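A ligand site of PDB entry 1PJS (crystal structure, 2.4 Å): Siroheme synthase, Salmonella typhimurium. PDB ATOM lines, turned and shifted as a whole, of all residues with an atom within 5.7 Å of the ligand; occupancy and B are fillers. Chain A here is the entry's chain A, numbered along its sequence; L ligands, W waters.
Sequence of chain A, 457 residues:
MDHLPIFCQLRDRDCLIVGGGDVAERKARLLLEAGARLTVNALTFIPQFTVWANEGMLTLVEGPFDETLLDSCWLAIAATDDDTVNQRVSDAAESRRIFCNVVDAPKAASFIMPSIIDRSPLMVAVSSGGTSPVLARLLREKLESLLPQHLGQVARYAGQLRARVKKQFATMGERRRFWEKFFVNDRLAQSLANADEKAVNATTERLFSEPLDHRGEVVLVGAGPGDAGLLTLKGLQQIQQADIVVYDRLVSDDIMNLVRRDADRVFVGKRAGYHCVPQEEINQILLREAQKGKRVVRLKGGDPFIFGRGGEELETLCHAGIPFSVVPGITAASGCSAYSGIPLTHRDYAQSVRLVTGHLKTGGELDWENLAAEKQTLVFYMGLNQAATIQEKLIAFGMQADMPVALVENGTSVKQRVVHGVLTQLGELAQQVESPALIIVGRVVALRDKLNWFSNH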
ATOM      1  N   PRO A 225     -10.037   9.222  -0.843  1.00  0.00           N
ATOM      2  CA  PRO A 225     -11.380   9.384  -0.235  1.00  0.00           C
ATOM      3  C   PRO A 225     -11.551   9.377   1.288  1.00  0.00           C
ATOM      4  O   PRO A 225     -12.562   9.878   1.789  1.00  0.00           O
ATOM      5  CB  PRO A 225     -12.188   8.275  -0.914  1.00  0.00           C
ATOM      6  CG  PRO A 225     -11.164   7.223  -1.195  1.00  0.00           C
ATOM      7  CD  PRO A 225      -9.987   8.011  -1.675  1.00  0.00           C
ATOM      8  N   GLY A 226     -10.597   8.822   2.039  1.00  0.00           N
ATOM      9  CA  GLY A 226     -10.756   8.819   3.483  1.00  0.00           C
ATOM     10  C   GLY A 226      -9.922   7.753   4.158  1.00  0.00           C
ATOM     11  O   GLY A 226      -9.229   8.030   5.136  1.00  0.00           O
ATOM     12  N   LEU A 250     -12.043  17.312   3.763  1.00  0.00           N
ATOM     13  CA  LEU A 250     -12.174  16.040   3.058  1.00  0.00           C
ATOM     14  C   LEU A 250     -10.928  15.192   3.215  1.00  0.00           C
ATOM     15  O   LEU A 250     -10.711  14.215   2.506  1.00  0.00           O
ATOM     16  CB  LEU A 250     -12.512  16.277   1.579  1.00  0.00           C
ATOM     17  CG  LEU A 250     -13.941  16.812   1.407  1.00  0.00           C
ATOM     18  CD1 LEU A 250     -14.370  16.697  -0.036  1.00  0.00           C
ATOM     19  CD2 LEU A 250     -14.887  16.001   2.276  1.00  0.00           C
ATOM     20  N   GLY A 301      -8.591  16.281  -0.521  1.00  0.00           N
ATOM     21  CA  GLY A 301      -9.299  15.014  -0.556  1.00  0.00           C
ATOM     22  C   GLY A 301      -9.291  14.444  -1.958  1.00  0.00           C
ATOM     23  O   GLY A 301      -9.213  15.184  -2.950  1.00  0.00           O
ATOM     24  N   GLY A 302      -9.368  13.117  -2.056  1.00  0.00           N
ATOM     25  CA  GLY A 302      -9.366  12.459  -3.349  1.00  0.00           C
ATOM     26  C   GLY A 302      -8.115  12.784  -4.147  1.00  0.00           C
ATOM     27  O   GLY A 302      -6.993  12.604  -3.659  1.00  0.00           O
ATOM     28  N   ASP A 303      -8.302  13.255  -5.381  1.00  0.00           N
ATOM     29  CA  ASP A 303      -7.195  13.618  -6.265  1.00  0.00           C
ATOM     30  C   ASP A 303      -7.270  15.128  -6.610  1.00  0.00           C
ATOM     31  O   ASP A 303      -8.317  15.638  -7.005  1.00  0.00           O
ATOM     32  CB  ASP A 303      -7.258  12.766  -7.539  1.00  0.00           C
ATOM     33  CG  ASP A 303      -6.282  13.243  -8.608  1.00  0.00           C
ATOM     34  OD1 ASP A 303      -5.118  13.528  -8.265  1.00  0.00           O
ATOM     35  OD2 ASP A 303      -6.689  13.325  -9.787  1.00  0.00           O
ATOM     36  N   PRO A 304      -6.140  15.845  -6.461  1.00  0.00           N
ATOM     37  CA  PRO A 304      -6.042  17.283  -6.738  1.00  0.00           C
ATOM     38  C   PRO A 304      -6.416  17.875  -8.108  1.00  0.00           C
ATOM     39  O   PRO A 304      -6.880  19.004  -8.181  1.00  0.00           O
ATOM     40  CB  PRO A 304      -4.597  17.609  -6.328  1.00  0.00           C
ATOM     41  CG  PRO A 304      -3.864  16.328  -6.524  1.00  0.00           C
ATOM     42  CD  PRO A 304      -4.846  15.304  -6.011  1.00  0.00           C
ATOM     43  N   ILE A 306      -8.775  16.759 -10.108  1.00  0.00           N
ATOM     44  CA  ILE A 306     -10.136  16.336 -10.427  1.00  0.00           C
ATOM     45  C   ILE A 306     -11.080  16.969  -9.407  1.00  0.00           C
ATOM     46  O   ILE A 306     -11.179  16.521  -8.272  1.00  0.00           O
ATOM     47  CB  ILE A 306     -10.289  14.787 -10.397  1.00  0.00           C
ATOM     48  CG1 ILE A 306      -9.368  14.156 -11.444  1.00  0.00           C
ATOM     49  CG2 ILE A 306     -11.755  14.404 -10.654  1.00  0.00           C
ATOM     50  CD1 ILE A 306      -9.543  12.680 -11.640  1.00  0.00           C
ATOM     51  N   PHE A 307     -11.744  18.029  -9.845  1.00  0.00           N
ATOM     52  CA  PHE A 307     -12.697  18.794  -9.036  1.00  0.00           C
ATOM     53  C   PHE A 307     -12.183  19.442  -7.756  1.00  0.00           C
ATOM     54  O   PHE A 307     -12.949  19.877  -6.901  1.00  0.00           O
ATOM     55  CB  PHE A 307     -13.938  17.953  -8.785  1.00  0.00           C
ATOM     56  CG  PHE A 307     -14.704  17.659 -10.041  1.00  0.00           C
ATOM     57  CD1 PHE A 307     -15.273  16.416 -10.264  1.00  0.00           C
ATOM     58  CD2 PHE A 307     -14.808  18.644 -11.040  1.00  0.00           C
ATOM     59  CE1 PHE A 307     -15.931  16.137 -11.464  1.00  0.00           C
ATOM     60  CE2 PHE A 307     -15.461  18.382 -12.226  1.00  0.00           C
ATOM     61  CZ  PHE A 307     -16.020  17.131 -12.447  1.00  0.00           C
ATOM     62  N   GLY A 308     -10.860  19.469  -7.605  1.00  0.00           N
ATOM     63  CA  GLY A 308     -10.295  20.166  -6.470  1.00  0.00           C
ATOM     64  C   GLY A 308      -9.978  21.452  -7.198  1.00  0.00           C
ATOM     65  O   GLY A 308     -10.531  21.685  -8.275  1.00  0.00           O
ATOM     66  N   ILE A 330      -6.129   8.638  -5.041  1.00  0.00           N
ATOM     67  CA  ILE A 330      -7.298   7.871  -5.432  1.00  0.00           C
ATOM     68  C   ILE A 330      -8.473   8.836  -5.432  1.00  0.00           C
ATOM     69  O   ILE A 330      -8.803   9.424  -4.393  1.00  0.00           O
ATOM     70  CB  ILE A 330      -7.571   6.741  -4.430  1.00  0.00           C
ATOM     71  CG1 ILE A 330      -6.353   5.803  -4.372  1.00  0.00           C
ATOM     72  CG2 ILE A 330      -8.841   5.991  -4.805  1.00  0.00           C
ATOM     73  CD1 ILE A 330      -5.983   5.183  -5.711  1.00  0.00           C
ATOM     74  N   THR A 331      -9.101   9.012  -6.593  1.00  0.00           N
ATOM     75  CA  THR A 331     -10.241   9.915  -6.698  1.00  0.00           C
ATOM     76  C   THR A 331     -11.422   9.281  -5.959  1.00  0.00           C
ATOM     77  O   THR A 331     -11.442   8.056  -5.748  1.00  0.00           O
ATOM     78  CB  THR A 331     -10.614  10.156  -8.166  1.00  0.00           C
ATOM     79  OG1 THR A 331     -11.305  11.408  -8.280  1.00  0.00           O
ATOM     80  CG2 THR A 331     -11.503   9.034  -8.679  1.00  0.00           C
ATOM     81  N   ALA A 332     -12.380  10.099  -5.565  1.00  0.00           N
ATOM     82  CA  ALA A 332     -13.540   9.610  -4.824  1.00  0.00           C
ATOM     83  C   ALA A 332     -14.310   8.599  -5.654  1.00  0.00           C
ATOM     84  O   ALA A 332     -14.820   7.604  -5.117  1.00  0.00           O
ATOM     85  CB  ALA A 332     -14.446  10.760  -4.438  1.00  0.00           C
ATOM     86  N   ALA A 333     -14.378   8.850  -6.957  1.00  0.00           N
ATOM     87  CA  ALA A 333     -15.074   7.987  -7.896  1.00  0.00           C
ATOM     88  C   ALA A 333     -14.495   6.572  -7.929  1.00  0.00           C
ATOM     89  O   ALA A 333     -15.232   5.604  -8.075  1.00  0.00           O
ATOM     90  CB  ALA A 333     -15.035   8.589  -9.285  1.00  0.00           C
ATOM     91  N   CYS A 336     -14.863   5.083  -3.830  1.00  0.00           N
ATOM     92  CA  CYS A 336     -16.242   4.739  -3.474  1.00  0.00           C
ATOM     93  C   CYS A 336     -16.789   3.572  -4.247  1.00  0.00           C
ATOM     94  O   CYS A 336     -17.315   2.620  -3.665  1.00  0.00           O
ATOM     95  CB  CYS A 336     -17.164   5.936  -3.675  1.00  0.00           C
ATOM     96  SG  CYS A 336     -16.884   7.214  -2.493  1.00  0.00           S
ATOM     97  N   PHE A 380     -21.396  11.512 -10.129  1.00  0.00           N
ATOM     98  CA  PHE A 380     -21.629  12.892  -9.740  1.00  0.00           C
ATOM     99  C   PHE A 380     -20.995  13.324  -8.423  1.00  0.00           C
ATOM    100  O   PHE A 380     -21.298  12.781  -7.353  1.00  0.00           O
ATOM    101  CB  PHE A 380     -23.127  13.187  -9.660  1.00  0.00           C
ATOM    102  CG  PHE A 380     -23.826  13.124 -10.980  1.00  0.00           C
ATOM    103  CD1 PHE A 380     -24.121  11.897 -11.566  1.00  0.00           C
ATOM    104  CD2 PHE A 380     -24.168  14.286 -11.645  1.00  0.00           C
ATOM    105  CE1 PHE A 380     -24.756  11.848 -12.791  1.00  0.00           C
ATOM    106  CE2 PHE A 380     -24.804  14.246 -12.869  1.00  0.00           C
ATOM    107  CZ  PHE A 380     -25.100  13.029 -13.453  1.00  0.00           C
ATOM    108  N   TYR A 381     -20.118  14.313  -8.508  1.00  0.00           N
ATOM    109  CA  TYR A 381     -19.468  14.862  -7.344  1.00  0.00           C
ATOM    110  C   TYR A 381     -20.337  16.089  -7.028  1.00  0.00           C
ATOM    111  O   TYR A 381     -20.872  16.726  -7.940  1.00  0.00           O
ATOM    112  CB  TYR A 381     -18.041  15.320  -7.676  1.00  0.00           C
ATOM    113  CG  TYR A 381     -16.964  14.242  -7.810  1.00  0.00           C
ATOM    114  CD1 TYR A 381     -17.036  13.266  -8.814  1.00  0.00           C
ATOM    115  CD2 TYR A 381     -15.844  14.243  -6.972  1.00  0.00           C
ATOM    116  CE1 TYR A 381     -15.992  12.321  -8.975  1.00  0.00           C
ATOM    117  CE2 TYR A 381     -14.814  13.315  -7.124  1.00  0.00           C
ATOM    118  CZ  TYR A 381     -14.886  12.361  -8.134  1.00  0.00           C
ATOM    119  OH  TYR A 381     -13.846  11.476  -8.296  1.00  0.00           O
ATOM    120  N   MET A 382     -20.480  16.397  -5.745  1.00  0.00           N
ATOM    121  CA  MET A 382     -21.223  17.564  -5.277  1.00  0.00           C
ATOM    122  C   MET A 382     -22.664  17.772  -5.787  1.00  0.00           C
ATOM    123  O   MET A 382     -23.003  18.886  -6.207  1.00  0.00           O
ATOM    124  CB  MET A 382     -20.417  18.826  -5.606  1.00  0.00           C
ATOM    125  CG  MET A 382     -18.954  18.759  -5.200  1.00  0.00           C
ATOM    126  SD  MET A 382     -18.055  20.278  -5.550  1.00  0.00           S
ATOM    127  CE  MET A 382     -17.673  20.054  -7.268  1.00  0.00           C
ATOM    128  N   GLY A 383     -23.513  16.759  -5.721  1.00  0.00           N
ATOM    129  CA  GLY A 383     -24.866  16.953  -6.209  1.00  0.00           C
ATOM    130  C   GLY A 383     -25.995  16.382  -5.379  1.00  0.00           C
ATOM    131  O   GLY A 383     -27.043  16.061  -5.928  1.00  0.00           O
ATOM    132  N   VAL A 408     -23.089   6.884  -2.510  1.00  0.00           N
ATOM    133  CA  VAL A 408     -22.117   6.449  -1.531  1.00  0.00           C
ATOM    134  C   VAL A 408     -21.786   7.549  -0.547  1.00  0.00           C
ATOM    135  O   VAL A 408     -21.309   8.617  -0.921  1.00  0.00           O
ATOM    136  CB  VAL A 408     -20.857   5.968  -2.242  1.00  0.00           C
ATOM    137  CG1 VAL A 408     -19.849   5.503  -1.237  1.00  0.00           C
ATOM    138  CG2 VAL A 408     -21.224   4.852  -3.208  1.00  0.00           C
ATOM    139  N   GLU A 409     -22.024   7.287   0.731  1.00  0.00           N
ATOM    140  CA  GLU A 409     -21.752   8.281   1.763  1.00  0.00           C
ATOM    141  C   GLU A 409     -20.510   7.915   2.558  1.00  0.00           C
ATOM    142  O   GLU A 409     -20.413   6.834   3.115  1.00  0.00           O
ATOM    143  CB  GLU A 409     -22.959   8.377   2.703  1.00  0.00           C
ATOM    144  CG  GLU A 409     -22.841   9.438   3.778  1.00  0.00           C
ATOM    145  CD  GLU A 409     -24.097   9.536   4.599  1.00  0.00           C
ATOM    146  OE1 GLU A 409     -25.152   9.822   4.002  1.00  0.00           O
ATOM    147  OE2 GLU A 409     -24.048   9.316   5.819  1.00  0.00           O
ATOM    148  N   ASN A 410     -19.565   8.850   2.609  1.00  0.00           N
ATOM    149  CA  ASN A 410     -18.311   8.630   3.328  1.00  0.00           C
ATOM    150  C   ASN A 410     -17.590   7.397   2.810  1.00  0.00           C
ATOM    151  O   ASN A 410     -17.214   6.509   3.578  1.00  0.00           O
ATOM    152  CB  ASN A 410     -18.578   8.485   4.820  1.00  0.00           C
ATOM    153  CG  ASN A 410     -19.017   9.783   5.462  1.00  0.00           C
ATOM    154  OD1 ASN A 410     -20.124   9.880   5.998  1.00  0.00           O
ATOM    155  ND2 ASN A 410     -18.153  10.794   5.420  1.00  0.00           N
ATOM    156  N   GLY A 411     -17.403   7.353   1.493  1.00  0.00           N
ATOM    157  CA  GLY A 411     -16.718   6.235   0.859  1.00  0.00           C
ATOM    158  C   GLY A 411     -15.356   5.935   1.446  1.00  0.00           C
ATOM    159  O   GLY A 411     -14.644   6.850   1.861  1.00  0.00           O
ATOM    160  N   THR A 412     -15.012   4.649   1.466  1.00  0.00           N
ATOM    161  CA  THR A 412     -13.748   4.114   1.982  1.00  0.00           C
ATOM    162  C   THR A 412     -13.600   4.249   3.485  1.00  0.00           C
ATOM    163  O   THR A 412     -12.679   3.664   4.074  1.00  0.00           O
ATOM    164  CB  THR A 412     -12.517   4.759   1.280  1.00  0.00           C
ATOM    165  OG1 THR A 412     -12.284   6.085   1.771  1.00  0.00           O
ATOM    166  CG2 THR A 412     -12.745   4.816  -0.211  1.00  0.00           C
ATOM    167  N   SER A 435     -24.115  14.567   2.829  1.00  0.00           N
ATOM    168  CA  SER A 435     -22.748  14.799   2.333  1.00  0.00           C
ATOM    169  C   SER A 435     -21.660  14.499   3.381  1.00  0.00           C
ATOM    170  O   SER A 435     -21.880  14.607   4.584  1.00  0.00           O
ATOM    171  CB  SER A 435     -22.638  16.240   1.838  1.00  0.00           C
ATOM    172  OG  SER A 435     -21.423  16.845   2.255  1.00  0.00           O
ATOM    173  N   PRO A 436     -20.441  14.128   2.921  1.00  0.00           N
ATOM    174  CA  PRO A 436     -20.052  13.969   1.514  1.00  0.00           C
ATOM    175  C   PRO A 436     -20.515  12.653   0.917  1.00  0.00           C
ATOM    176  O   PRO A 436     -20.230  11.568   1.442  1.00  0.00           O
ATOM    177  CB  PRO A 436     -18.539  14.093   1.567  1.00  0.00           C
ATOM    178  CG  PRO A 436     -18.214  13.417   2.845  1.00  0.00           C
ATOM    179  CD  PRO A 436     -19.276  13.925   3.797  1.00  0.00           C
ATOM    180  N   ALA A 437     -21.224  12.751  -0.197  1.00  0.00           N
ATOM    181  CA  ALA A 437     -21.715  11.566  -0.873  1.00  0.00           C
ATOM    182  C   ALA A 437     -21.477  11.667  -2.360  1.00  0.00           C
ATOM    183  O   ALA A 437     -21.325  12.755  -2.909  1.00  0.00           O
ATOM    184  CB  ALA A 437     -23.192  11.383  -0.579  1.00  0.00           C
ATOM    185  N   LEU A 438     -21.457  10.514  -3.001  1.00  0.00           N
ATOM    186  CA  LEU A 438     -21.234  10.410  -4.424  1.00  0.00           C
ATOM    187  C   LEU A 438     -22.436   9.703  -5.035  1.00  0.00           C
ATOM    188  O   LEU A 438     -23.068   8.879  -4.375  1.00  0.00           O
ATOM    189  CB  LEU A 438     -19.970   9.597  -4.688  1.00  0.00           C
ATOM    190  CG  LEU A 438     -18.968  10.206  -5.663  1.00  0.00           C
ATOM    191  CD1 LEU A 438     -17.768   9.289  -5.827  1.00  0.00           C
ATOM    192  CD2 LEU A 438     -19.666  10.428  -6.983  1.00  0.00           C
HETATM  193  N1  LIG L   1     -10.785  15.947  -5.604  1.00  0.00           N
HETATM  194  C1  LIG L   1     -11.752  15.004  -5.019  1.00  0.00           C
HETATM  195  C2  LIG L   1     -13.168  15.568  -5.171  1.00  0.00           C
HETATM  196  C3  LIG L   1     -13.333  16.877  -4.396  1.00  0.00           C
HETATM  197  S1  LIG L   1     -14.940  17.728  -4.709  1.00  0.00           S
HETATM  198  C4  LIG L   1     -11.645  13.638  -5.726  1.00  0.00           C
HETATM  199  O1  LIG L   1     -10.816  13.539  -6.659  1.00  0.00           O
HETATM  200  O2  LIG L   1     -12.405  12.726  -5.319  1.00  0.00           O
HETATM  201  C5  LIG L   1     -15.928  17.193  -3.273  1.00  0.00           C
HETATM  202  C6  LIG L   1     -16.798  15.970  -3.578  1.00  0.00           C
HETATM  203  O3  LIG L   1     -16.040  14.725  -3.728  1.00  0.00           O
HETATM  204  C7  LIG L   1     -17.810  15.659  -2.499  1.00  0.00           C
HETATM  205  O4  LIG L   1     -18.929  16.518  -2.628  1.00  0.00           O
HETATM  206  C8  LIG L   1     -18.218  14.260  -2.841  1.00  0.00           C
HETATM  207  O5  LIG L   1     -19.168  14.282  -3.901  1.00  0.00           O
HETATM  208  C9  LIG L   1     -16.910  13.597  -3.319  1.00  0.00           C
HETATM  209  N2  LIG L   1     -16.267  12.857  -2.184  1.00  0.00           N
HETATM  210  C10 LIG L   1     -15.093  13.146  -1.595  1.00  0.00           C
HETATM  211  N3  LIG L   1     -14.854  12.224  -0.640  1.00  0.00           N
HETATM  212  C11 LIG L   1     -15.873  11.364  -0.636  1.00  0.00           C
HETATM  213  C12 LIG L   1     -16.175  10.228   0.114  1.00  0.00           C
HETATM  214  N4  LIG L   1     -15.326   9.796   1.048  1.00  0.00           N
HETATM  215  N5  LIG L   1     -17.322   9.553  -0.127  1.00  0.00           N
HETATM  216  C13 LIG L   1     -18.176   9.966  -1.076  1.00  0.00           C
HETATM  217  N6  LIG L   1     -17.906  11.055  -1.812  1.00  0.00           N
HETATM  218  C14 LIG L   1     -16.760  11.756  -1.609  1.00  0.00           C
HETATM  219  O   HOH W   1     -21.709  15.741  -0.946  1.00  0.00           O
HETATM  220  O   HOH W   2     -12.421  12.959   0.571  1.00  0.00           O
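O of Gly 301 lies within hydrogen-bond range of N1 of the ligand, at 3.2 Å. The backbone carbonyl oxygen (O) of Gly 411 sits at hydrogen-bond distance from a nitrogen (N4) of the ligand (3.1 Å). An oxygen (O5) of the ligand sits at hydrogen-bond distance from the backbone NH (N) of Met 382 (3.1 Å). O2 of the ligand sits at hydrogen-bond distance from N of Ala 332 (2.6 Å). The backbone carbonyl oxygen (O) of Pro 225 is in hydrogen-bond range of a nitrogen (N4) of the ligand. O of Ile 306 is in hydrogen-bond range of N1 of the ligand, 2.8 Å away. N of Asp 303 lies within hydrogen-bond range of O1 of the ligand (2.8 Å). N of Gly 411 sits at hydrogen-bond distance from N5 of the ligand (2.7 Å). O of Ala 437 is in hydrogen-bond range of O5 of the ligand (2.8 Å). SG of Cys 336 sits close to N5 of the ligand, at 3.4 Å. O1 of the ligand sits at hydrogen-bond distance from OG1 of Thr 331 (2.7 Å). A nitrogen (N1) of the ligand sits at hydrogen-bond distance from the backbone carbonyl oxygen (O) of Asp 303.
Water W1 lies within hydrogen-bond range of the backbone NH of Ala 437, an oxygen (O4) of the ligand and the side-chain hydroxyl of Ser 435.
The backbone carbonyl oxygen (O) of Ala 332 sits close to the side-chain sulfur (SG) of Cys 336 (3.4 Å). O of Leu 438 lies within hydrogen-bond range of N of Val 408 (2.7 Å). N of Ala 332 is in hydrogen-bond range of OH of Tyr 381, at 3.4 Å. N of Ala 333 is in hydrogen-bond range of OH of Tyr 381 (3.0 Å). The side-chain hydroxyl of Thr 331 is in hydrogen-bond range of the side-chain hydroxyl of Tyr 381, 2.5 Å away. The backbone carbonyl oxygen (O) of Pro 436 sits at hydrogen-bond distance from the backbone NH (N) of Asn 410 (3.0 Å).
A sulfur (S1) of the ligand sits close to the backbone carbonyl oxygen (O) of Phe 307 (3.7 Å). Residues that only touch the ligand: Tyr 381, Val 408, Gly 302, Asn 410, Pro 436, Leu 250 and Leu 438. Hydrophobic or aromatic side chains within 4 Å of the ligand: Leu 250, Ile 306, Ala 332, Tyr 381, Met 382 and Leu 438. Of the 28 residues printed, 18 come within 4 Å of the ligand. The nearest printed residue that does not touch the ligand is Gly 308 (4.1 Å).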
